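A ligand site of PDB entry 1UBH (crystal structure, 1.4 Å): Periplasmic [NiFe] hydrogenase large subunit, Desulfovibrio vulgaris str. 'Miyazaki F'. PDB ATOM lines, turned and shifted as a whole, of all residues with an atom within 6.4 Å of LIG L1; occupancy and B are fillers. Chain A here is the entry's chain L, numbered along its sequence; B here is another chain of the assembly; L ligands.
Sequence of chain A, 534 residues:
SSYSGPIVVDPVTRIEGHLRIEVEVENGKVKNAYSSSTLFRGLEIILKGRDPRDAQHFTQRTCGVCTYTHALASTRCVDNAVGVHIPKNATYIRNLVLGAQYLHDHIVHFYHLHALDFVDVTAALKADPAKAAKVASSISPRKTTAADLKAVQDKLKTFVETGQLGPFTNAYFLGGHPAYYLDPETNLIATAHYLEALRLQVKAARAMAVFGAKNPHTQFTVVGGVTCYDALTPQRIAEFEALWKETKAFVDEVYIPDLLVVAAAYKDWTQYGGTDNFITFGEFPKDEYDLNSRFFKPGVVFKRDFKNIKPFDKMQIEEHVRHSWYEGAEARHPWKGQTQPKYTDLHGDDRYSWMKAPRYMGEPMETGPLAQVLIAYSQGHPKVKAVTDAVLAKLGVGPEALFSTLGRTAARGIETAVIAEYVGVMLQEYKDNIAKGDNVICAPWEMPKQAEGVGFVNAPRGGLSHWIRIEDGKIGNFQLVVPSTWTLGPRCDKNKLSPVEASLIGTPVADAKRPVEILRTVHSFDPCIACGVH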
ATOM      1  N   GLU A  16     -18.297 -25.438  -4.826  1.00  0.00           N
ATOM      2  CA  GLU A  16     -18.379 -24.004  -4.987  1.00  0.00           C
ATOM      3  C   GLU A  16     -19.807 -23.699  -5.473  1.00  0.00           C
ATOM      4  O   GLU A  16     -20.272 -24.207  -6.457  1.00  0.00           O
ATOM      5  CB  GLU A  16     -17.280 -23.460  -5.902  1.00  0.00           C
ATOM      6  CG  GLU A  16     -17.067 -21.957  -5.963  1.00  0.00           C
ATOM      7  CD  GLU A  16     -18.215 -21.130  -6.472  1.00  0.00           C
ATOM      8  OE1 GLU A  16     -18.638 -20.083  -5.967  1.00  0.00           O
ATOM      9  OE2 GLU A  16     -18.884 -21.774  -7.366  1.00  0.00           O
ATOM     10  N   THR A  62     -15.167 -14.740 -11.846  1.00  0.00           N
ATOM     11  CA  THR A  62     -16.106 -15.871 -12.056  1.00  0.00           C
ATOM     12  C   THR A  62     -16.015 -16.832 -10.887  1.00  0.00           C
ATOM     13  O   THR A  62     -17.009 -17.356 -10.399  1.00  0.00           O
ATOM     14  CB  THR A  62     -15.829 -16.625 -13.370  1.00  0.00           C
ATOM     15  OG1 THR A  62     -16.067 -15.719 -14.478  1.00  0.00           O
ATOM     16  CG2 THR A  62     -16.685 -17.848 -13.503  1.00  0.00           C
ATOM     17  N   CYS A  63     -14.772 -17.085 -10.420  1.00  0.00           N
ATOM     18  CA  CYS A  63     -14.559 -18.099  -9.430  1.00  0.00           C
ATOM     19  C   CYS A  63     -13.195 -17.960  -8.745  1.00  0.00           C
ATOM     20  O   CYS A  63     -12.145 -17.785  -9.399  1.00  0.00           O
ATOM     21  CB  CYS A  63     -14.680 -19.454 -10.111  1.00  0.00           C
ATOM     22  SG  CYS A  63     -14.572 -20.814  -8.879  1.00  0.00           S
ATOM     23  N   GLY A  64     -13.265 -18.046  -7.411  1.00  0.00           N
ATOM     24  CA  GLY A  64     -12.106 -17.991  -6.551  1.00  0.00           C
ATOM     25  C   GLY A  64     -11.584 -19.317  -6.103  1.00  0.00           C
ATOM     26  O   GLY A  64     -10.523 -19.368  -5.456  1.00  0.00           O
ATOM     27  N   VAL A  65     -12.302 -20.385  -6.434  1.00  0.00           N
ATOM     28  CA  VAL A  65     -11.820 -21.745  -6.179  1.00  0.00           C
ATOM     29  C   VAL A  65     -10.886 -22.061  -7.331  1.00  0.00           C
ATOM     30  O   VAL A  65      -9.685 -22.283  -7.151  1.00  0.00           O
ATOM     31  CB  VAL A  65     -12.965 -22.743  -6.024  1.00  0.00           C
ATOM     32  CG1 VAL A  65     -12.431 -24.153  -5.907  1.00  0.00           C
ATOM     33  CG2 VAL A  65     -13.780 -22.385  -4.785  1.00  0.00           C
ATOM     34  N   CYS A  66     -11.454 -22.028  -8.542  1.00  0.00           N
ATOM     35  CA  CYS A  66     -10.629 -22.125  -9.730  1.00  0.00           C
ATOM     36  C   CYS A  66     -10.123 -20.738 -10.121  1.00  0.00           C
ATOM     37  O   CYS A  66     -10.243 -20.216 -11.207  1.00  0.00           O
ATOM     38  CB  CYS A  66     -11.326 -22.837 -10.857  1.00  0.00           C
ATOM     39  SG  CYS A  66     -12.746 -22.023 -11.569  1.00  0.00           S
ATOM     40  N   THR A  67      -9.533 -20.098  -9.108  1.00  0.00           N
ATOM     41  CA  THR A  67      -8.886 -18.828  -9.304  1.00  0.00           C
ATOM     42  C   THR A  67      -7.839 -19.070 -10.352  1.00  0.00           C
ATOM     43  O   THR A  67      -7.324 -20.129 -10.727  1.00  0.00           O
ATOM     44  CB  THR A  67      -8.303 -18.305  -7.973  1.00  0.00           C
ATOM     45  OG1 THR A  67      -8.039 -16.969  -8.302  1.00  0.00           O
ATOM     46  CG2 THR A  67      -7.057 -19.062  -7.479  1.00  0.00           C
ATOM     47  N   THR A  69      -7.660 -19.430 -13.428  1.00  0.00           N
ATOM     48  CA  THR A  69      -8.035 -20.092 -14.675  1.00  0.00           C
ATOM     49  C   THR A  69      -8.770 -19.134 -15.626  1.00  0.00           C
ATOM     50  O   THR A  69      -8.473 -19.197 -16.841  1.00  0.00           O
ATOM     51  CB  THR A  69      -8.899 -21.363 -14.471  1.00  0.00           C
ATOM     52  OG1 THR A  69     -10.144 -21.050 -13.900  1.00  0.00           O
ATOM     53  CG2 THR A  69      -8.171 -22.385 -13.578  1.00  0.00           C
ATOM     54  N   HIS A  70      -9.643 -18.297 -15.089  1.00  0.00           N
ATOM     55  CA  HIS A  70     -10.393 -17.412 -15.961  1.00  0.00           C
ATOM     56  C   HIS A  70      -9.554 -16.206 -16.429  1.00  0.00           C
ATOM     57  O   HIS A  70      -9.762 -15.724 -17.532  1.00  0.00           O
ATOM     58  CB  HIS A  70     -11.721 -16.919 -15.333  1.00  0.00           C
ATOM     59  CG  HIS A  70     -12.713 -18.028 -15.182  1.00  0.00           C
ATOM     60  ND1 HIS A  70     -13.518 -18.433 -16.211  1.00  0.00           N
ATOM     61  CD2 HIS A  70     -13.004 -18.818 -14.116  1.00  0.00           C
ATOM     62  CE1 HIS A  70     -14.275 -19.440 -15.771  1.00  0.00           C
ATOM     63  NE2 HIS A  70     -13.987 -19.707 -14.474  1.00  0.00           N
ATOM     64  N   GLN A 101      -1.998 -24.441  -9.556  1.00  0.00           N
ATOM     65  CA  GLN A 101      -3.433 -24.373  -9.330  1.00  0.00           C
ATOM     66  C   GLN A 101      -4.056 -25.779  -9.300  1.00  0.00           C
ATOM     67  O   GLN A 101      -4.854 -26.098  -8.436  1.00  0.00           O
ATOM     68  CB  GLN A 101      -4.131 -23.479 -10.384  1.00  0.00           C
ATOM     69  CG  GLN A 101      -5.657 -23.527 -10.345  1.00  0.00           C
ATOM     70  CD  GLN A 101      -6.280 -23.050  -9.060  1.00  0.00           C
ATOM     71  OE1 GLN A 101      -5.739 -22.229  -8.323  1.00  0.00           O
ATOM     72  NE2 GLN A 101      -7.484 -23.583  -8.783  1.00  0.00           N
ATOM     73  N   ASP A 105      -5.947 -27.255  -6.034  1.00  0.00           N
ATOM     74  CA  ASP A 105      -7.393 -27.459  -6.204  1.00  0.00           C
ATOM     75  C   ASP A 105      -7.825 -28.884  -5.946  1.00  0.00           C
ATOM     76  O   ASP A 105      -8.740 -29.181  -5.165  1.00  0.00           O
ATOM     77  CB  ASP A 105      -7.750 -26.967  -7.621  1.00  0.00           C
ATOM     78  CG  ASP A 105      -9.201 -26.635  -7.884  1.00  0.00           C
ATOM     79  OD1 ASP A 105     -10.037 -27.232  -7.142  1.00  0.00           O
ATOM     80  OD2 ASP A 105      -9.459 -25.832  -8.825  1.00  0.00           O
ATOM     81  N   VAL A 457      -8.605 -23.139 -21.995  1.00  0.00           N
ATOM     82  CA  VAL A 457      -7.893 -23.648 -20.829  1.00  0.00           C
ATOM     83  C   VAL A 457      -8.512 -24.993 -20.451  1.00  0.00           C
ATOM     84  O   VAL A 457      -9.750 -25.077 -20.431  1.00  0.00           O
ATOM     85  CB  VAL A 457      -7.993 -22.679 -19.637  1.00  0.00           C
ATOM     86  CG1 VAL A 457      -7.365 -23.233 -18.367  1.00  0.00           C
ATOM     87  CG2 VAL A 457      -7.312 -21.355 -20.005  1.00  0.00           C
ATOM     88  N   ALA A 459      -9.093 -26.553 -17.350  1.00  0.00           N
ATOM     89  CA  ALA A 459      -9.034 -26.183 -15.958  1.00  0.00           C
ATOM     90  C   ALA A 459      -9.160 -27.425 -15.077  1.00  0.00           C
ATOM     91  O   ALA A 459      -9.400 -28.507 -15.641  1.00  0.00           O
ATOM     92  CB  ALA A 459     -10.162 -25.186 -15.690  1.00  0.00           C
ATOM     93  N   PRO A 460      -8.973 -27.339 -13.775  1.00  0.00           N
ATOM     94  CA  PRO A 460      -9.169 -28.555 -12.944  1.00  0.00           C
ATOM     95  C   PRO A 460     -10.518 -29.261 -13.099  1.00  0.00           C
ATOM     96  O   PRO A 460     -10.623 -30.466 -12.791  1.00  0.00           O
ATOM     97  CB  PRO A 460      -8.962 -27.979 -11.512  1.00  0.00           C
ATOM     98  CG  PRO A 460      -7.947 -26.882 -11.748  1.00  0.00           C
ATOM     99  CD  PRO A 460      -8.519 -26.202 -12.973  1.00  0.00           C
ATOM    100  N   ARG A 461     -11.563 -28.583 -13.569  1.00  0.00           N
ATOM    101  CA  ARG A 461     -12.867 -29.217 -13.811  1.00  0.00           C
ATOM    102  C   ARG A 461     -13.182 -29.441 -15.292  1.00  0.00           C
ATOM    103  O   ARG A 461     -14.238 -29.958 -15.598  1.00  0.00           O
ATOM    104  CB  ARG A 461     -13.970 -28.388 -13.143  1.00  0.00           C
ATOM    105  CG  ARG A 461     -13.869 -28.420 -11.649  1.00  0.00           C
ATOM    106  CD  ARG A 461     -14.584 -27.244 -10.932  1.00  0.00           C
ATOM    107  NE  ARG A 461     -14.234 -27.381  -9.523  1.00  0.00           N
ATOM    108  CZ  ARG A 461     -13.064 -27.017  -9.002  1.00  0.00           C
ATOM    109  NH1 ARG A 461     -12.151 -26.429  -9.744  1.00  0.00           N
ATOM    110  NH2 ARG A 461     -12.816 -27.194  -7.718  1.00  0.00           N
ATOM    111  N   GLY A 462     -12.250 -29.051 -16.185  1.00  0.00           N
ATOM    112  CA  GLY A 462     -12.328 -29.380 -17.578  1.00  0.00           C
ATOM    113  C   GLY A 462     -12.211 -28.234 -18.552  1.00  0.00           C
ATOM    114  O   GLY A 462     -11.562 -27.220 -18.279  1.00  0.00           O
ATOM    115  N   GLY A 463     -12.873 -28.405 -19.719  1.00  0.00           N
ATOM    116  CA  GLY A 463     -12.638 -27.524 -20.821  1.00  0.00           C
ATOM    117  C   GLY A 463     -13.298 -26.158 -20.653  1.00  0.00           C
ATOM    118  O   GLY A 463     -14.517 -26.059 -20.718  1.00  0.00           O
ATOM    119  N   LEU A 464     -12.478 -25.126 -20.448  1.00  0.00           N
ATOM    120  CA  LEU A 464     -12.906 -23.755 -20.349  1.00  0.00           C
ATOM    121  C   LEU A 464     -12.609 -22.957 -21.591  1.00  0.00           C
ATOM    122  O   LEU A 464     -11.502 -23.062 -22.112  1.00  0.00           O
ATOM    123  CB  LEU A 464     -12.140 -23.132 -19.177  1.00  0.00           C
ATOM    124  CG  LEU A 464     -12.278 -21.629 -18.965  1.00  0.00           C
ATOM    125  CD1 LEU A 464     -13.735 -21.255 -18.721  1.00  0.00           C
ATOM    126  CD2 LEU A 464     -11.381 -21.154 -17.822  1.00  0.00           C
ATOM    127  N   VAL A 481     -17.863 -20.176 -21.548  1.00  0.00           N
ATOM    128  CA  VAL A 481     -18.430 -21.504 -21.584  1.00  0.00           C
ATOM    129  C   VAL A 481     -17.508 -22.324 -20.670  1.00  0.00           C
ATOM    130  O   VAL A 481     -16.336 -22.545 -20.984  1.00  0.00           O
ATOM    131  CB  VAL A 481     -18.492 -22.136 -22.973  1.00  0.00           C
ATOM    132  CG1 VAL A 481     -19.176 -23.515 -22.903  1.00  0.00           C
ATOM    133  CG2 VAL A 481     -19.184 -21.192 -23.926  1.00  0.00           C
ATOM    134  N   VAL A 482     -18.056 -22.727 -19.521  1.00  0.00           N
ATOM    135  CA  VAL A 482     -17.156 -23.154 -18.456  1.00  0.00           C
ATOM    136  C   VAL A 482     -17.311 -24.623 -18.178  1.00  0.00           C
ATOM    137  O   VAL A 482     -18.355 -25.175 -18.486  1.00  0.00           O
ATOM    138  CB  VAL A 482     -17.510 -22.241 -17.260  1.00  0.00           C
ATOM    139  CG1 VAL A 482     -16.626 -22.445 -16.061  1.00  0.00           C
ATOM    140  CG2 VAL A 482     -17.398 -20.770 -17.639  1.00  0.00           C
ATOM    141  N   PRO A 483     -16.316 -25.343 -17.678  1.00  0.00           N
ATOM    142  CA  PRO A 483     -16.464 -26.798 -17.488  1.00  0.00           C
ATOM    143  C   PRO A 483     -17.703 -27.219 -16.717  1.00  0.00           C
ATOM    144  O   PRO A 483     -18.418 -28.117 -17.197  1.00  0.00           O
ATOM    145  CB  PRO A 483     -15.175 -27.249 -16.777  1.00  0.00           C
ATOM    146  CG  PRO A 483     -14.353 -26.026 -16.592  1.00  0.00           C
ATOM    147  CD  PRO A 483     -14.967 -24.928 -17.381  1.00  0.00           C
ATOM    148  N   SER A 484     -18.032 -26.568 -15.586  1.00  0.00           N
ATOM    149  CA  SER A 484     -19.232 -26.993 -14.888  1.00  0.00           C
ATOM    150  C   SER A 484     -20.505 -26.674 -15.661  1.00  0.00           C
ATOM    151  O   SER A 484     -21.537 -27.285 -15.355  1.00  0.00           O
ATOM    152  CB  SER A 484     -19.273 -26.346 -13.524  1.00  0.00           C
ATOM    153  OG  SER A 484     -18.312 -26.837 -12.583  1.00  0.00           O
ATOM    154  N   THR A 485     -20.427 -25.748 -16.621  1.00  0.00           N
ATOM    155  CA  THR A 485     -21.596 -25.502 -17.469  1.00  0.00           C
ATOM    156  C   THR A 485     -21.860 -26.759 -18.277  1.00  0.00           C
ATOM    157  O   THR A 485     -22.963 -27.254 -18.412  1.00  0.00           O
ATOM    158  CB  THR A 485     -21.392 -24.320 -18.438  1.00  0.00           C
ATOM    159  OG1 THR A 485     -20.680 -23.276 -17.787  1.00  0.00           O
ATOM    160  CG2 THR A 485     -22.717 -23.831 -18.968  1.00  0.00           C
ATOM    161  N   ASP A 526     -16.984 -32.452  -8.996  1.00  0.00           N
ATOM    162  CA  ASP A 526     -16.369 -31.258  -8.430  1.00  0.00           C
ATOM    163  C   ASP A 526     -17.058 -30.001  -8.979  1.00  0.00           C
ATOM    164  O   ASP A 526     -16.501 -29.127  -9.657  1.00  0.00           O
ATOM    165  CB  ASP A 526     -14.880 -31.308  -8.714  1.00  0.00           C
ATOM    166  CG  ASP A 526     -14.003 -30.217  -8.188  1.00  0.00           C
ATOM    167  OD1 ASP A 526     -12.840 -30.171  -8.681  1.00  0.00           O
ATOM    168  OD2 ASP A 526     -14.465 -29.443  -7.330  1.00  0.00           O
ATOM    169  N   PRO A 527     -18.339 -29.861  -8.684  1.00  0.00           N
ATOM    170  CA  PRO A 527     -19.125 -28.756  -9.239  1.00  0.00           C
ATOM    171  C   PRO A 527     -18.667 -27.381  -8.787  1.00  0.00           C
ATOM    172  O   PRO A 527     -18.308 -27.162  -7.643  1.00  0.00           O
ATOM    173  CB  PRO A 527     -20.530 -28.993  -8.660  1.00  0.00           C
ATOM    174  CG  PRO A 527     -20.581 -30.444  -8.346  1.00  0.00           C
ATOM    175  CD  PRO A 527     -19.167 -30.730  -7.815  1.00  0.00           C
ATOM    176  N   CYS A 528     -18.815 -26.433  -9.703  1.00  0.00           N
ATOM    177  CA  CYS A 528     -18.534 -25.037  -9.433  1.00  0.00           C
ATOM    178  C   CYS A 528     -19.629 -24.200 -10.088  1.00  0.00           C
ATOM    179  O   CYS A 528     -19.607 -24.054 -11.303  1.00  0.00           O
ATOM    180  CB  CYS A 528     -17.145 -24.702  -9.960  1.00  0.00           C
ATOM    181  SG  CYS A 528     -16.722 -23.018  -9.484  1.00  0.00           S
ATOM    182  N   ILE A 529     -20.562 -23.727  -9.284  1.00  0.00           N
ATOM    183  CA  ILE A 529     -21.750 -23.087  -9.844  1.00  0.00           C
ATOM    184  C   ILE A 529     -21.514 -21.617 -10.180  1.00  0.00           C
ATOM    185  O   ILE A 529     -22.147 -21.089 -11.107  1.00  0.00           O
ATOM    186  CB  ILE A 529     -22.972 -23.240  -8.918  1.00  0.00           C
ATOM    187  CG1 ILE A 529     -23.105 -24.669  -8.419  1.00  0.00           C
ATOM    188  CG2 ILE A 529     -24.243 -22.750  -9.583  1.00  0.00           C
ATOM    189  CD1 ILE A 529     -23.158 -25.753  -9.460  1.00  0.00           C
ATOM    190  N   ALA A 530     -20.605 -20.940  -9.524  1.00  0.00           N
ATOM    191  CA  ALA A 530     -20.214 -19.607  -9.930  1.00  0.00           C
ATOM    192  C   ALA A 530     -19.542 -19.690 -11.311  1.00  0.00           C
ATOM    193  O   ALA A 530     -19.831 -18.905 -12.216  1.00  0.00           O
ATOM    194  CB  ALA A 530     -19.284 -19.031  -8.885  1.00  0.00           C
ATOM    195  N   CYS A 531     -18.671 -20.679 -11.486  1.00  0.00           N
ATOM    196  CA  CYS A 531     -18.127 -20.962 -12.796  1.00  0.00           C
ATOM    197  C   CYS A 531     -19.207 -21.270 -13.805  1.00  0.00           C
ATOM    198  O   CYS A 531     -19.246 -20.746 -14.911  1.00  0.00           O
ATOM    199  CB  CYS A 531     -17.219 -22.230 -12.680  1.00  0.00           C
ATOM    200  SG  CYS A 531     -15.522 -21.731 -12.417  1.00  0.00           S
ATOM    201  N   GLY A 532     -20.140 -22.178 -13.441  1.00  0.00           N
ATOM    202  CA  GLY A 532     -21.037 -22.665 -14.466  1.00  0.00           C
ATOM    203  C   GLY A 532     -21.985 -21.593 -14.940  1.00  0.00           C
ATOM    204  O   GLY A 532     -22.341 -21.630 -16.130  1.00  0.00           O
ATOM    205  N   CYS B  17     -17.870 -15.413  -5.526  1.00  0.00           N
ATOM    206  CA  CYS B  17     -17.077 -16.338  -6.320  1.00  0.00           C
ATOM    207  C   CYS B  17     -16.319 -17.338  -5.450  1.00  0.00           C
ATOM    208  O   CYS B  17     -15.631 -18.196  -6.002  1.00  0.00           O
ATOM    209  CB  CYS B  17     -16.089 -15.542  -7.155  1.00  0.00           C
ATOM    210  SG  CYS B  17     -14.602 -14.996  -6.258  1.00  0.00           S
HETATM  211 NI1  LIG L   1     -14.670 -22.534 -10.397  1.00  0.00          NI
HETATM  212 FE1  LIG L   1     -14.017 -23.443 -12.765  1.00  0.00          FE
HETATM  213  C1  LIG L   1     -15.487 -24.670 -13.332  1.00  0.00           C
HETATM  214  C2  LIG L   1     -12.777 -24.818 -12.732  1.00  0.00           C
HETATM  215  C3  LIG L   1     -13.507 -23.127 -14.413  1.00  0.00           C
HETATM  216  O1  LIG L   1     -16.305 -25.446 -13.589  1.00  0.00           O
HETATM  217  O2  LIG L   1     -11.961 -25.665 -12.759  1.00  0.00           O
HETATM  218  O3  LIG L   1     -13.141 -22.918 -15.487  1.00  0.00           O
HETATM  219  C1  LG2 L   2     -14.073 -23.944  -9.618  1.00  0.00           C
HETATM  220  O1  LG2 L   2     -14.115 -24.379  -8.565  1.00  0.00           O
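NH2 of Arg 461 is in salt-bridge range of OD2 of Asp 526, 2.8 Å away. The side-chain hydroxyl of Thr 485 is in hydrogen-bond range of the backbone carbonyl oxygen of Val 482, 3.1 Å away. The backbone NH (N) of Leu 464 is in hydrogen-bond range of the backbone carbonyl oxygen (O) of Val 457, 2.7 Å away. The backbone NH of Val 65 lies close to the side-chain sulfur of Cys 63, 3.4 Å away. OD1 of Asp 105 is in salt-bridge range of NH2 of Arg 461 (2.8 Å). The side-chain sulfur (SG) of Cys 528 lies close to the side-chain carboxylate (OE2) of Glu 16 (3.3 Å). The side-chain hydroxyl (OG) of Ser 484 is in hydrogen-bond range of the backbone NH (N) of Cys 528, 3.0 Å away. The side-chain sulfur of Cys 531 lies close to a ring nitrogen (NE2) of His 70 (3.3 Å).
An iron atom (FE1) of LIG L1 is bound by the side-chain sulfur of Cys 531, 2.3 Å away. The side-chain sulfur (SG) of Cys 63 sits close to an oxygen (O1) of LG2 L2, 3.6 Å away. SG of Cys 528 lies close to O1 of LG2 L2 (3.1 Å). O3 of LIG L1 sits close to NE2 of His 70. NH1 of Arg 461 sits close to O1 of LG2 L2, at 3.1 Å. A nickel atom (NI1) of LIG L1 is bound by the side-chain sulfur of Cys 528. OG of Ser 484 sits at hydrogen-bond distance from O1 of LIG L1 (2.6 Å). An oxygen (O2) of LIG L1 is in hydrogen-bond range of the backbone NH (N) of Arg 461 (3.1 Å). The backbone NH of Ser 484 is in hydrogen-bond range of an oxygen (O1) of LIG L1, 2.9 Å away. The side-chain sulfur (SG) of Cys 66 binds an iron atom (FE1) of LIG L1, at 2.2 Å. The guanidinium group of Arg 461 lies within hydrogen-bond range of an oxygen (O2) of LIG L1, 3.1 Å away. NI1 of LIG L1 is bound by SG of Cys 63, at 2.3 Å.
Residues that only touch LIG L1: Pro 483, Leu 464, Ala 459, Pro 460, Val 482 and Thr 69. Hydrophobic or aromatic side chains within 4 Å of LIG L1: His 70, Ala 459, Pro 460, Leu 464, Val 482 and Pro 483. Of the 31 residues printed, 13 come within 4 Å of LIG L1. Along chain A the residues within 4 Å of LIG L1 span positions 63 to 531. The nearest printed residue that does not touch LIG L1 is Asp 105 (4.7 Å).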
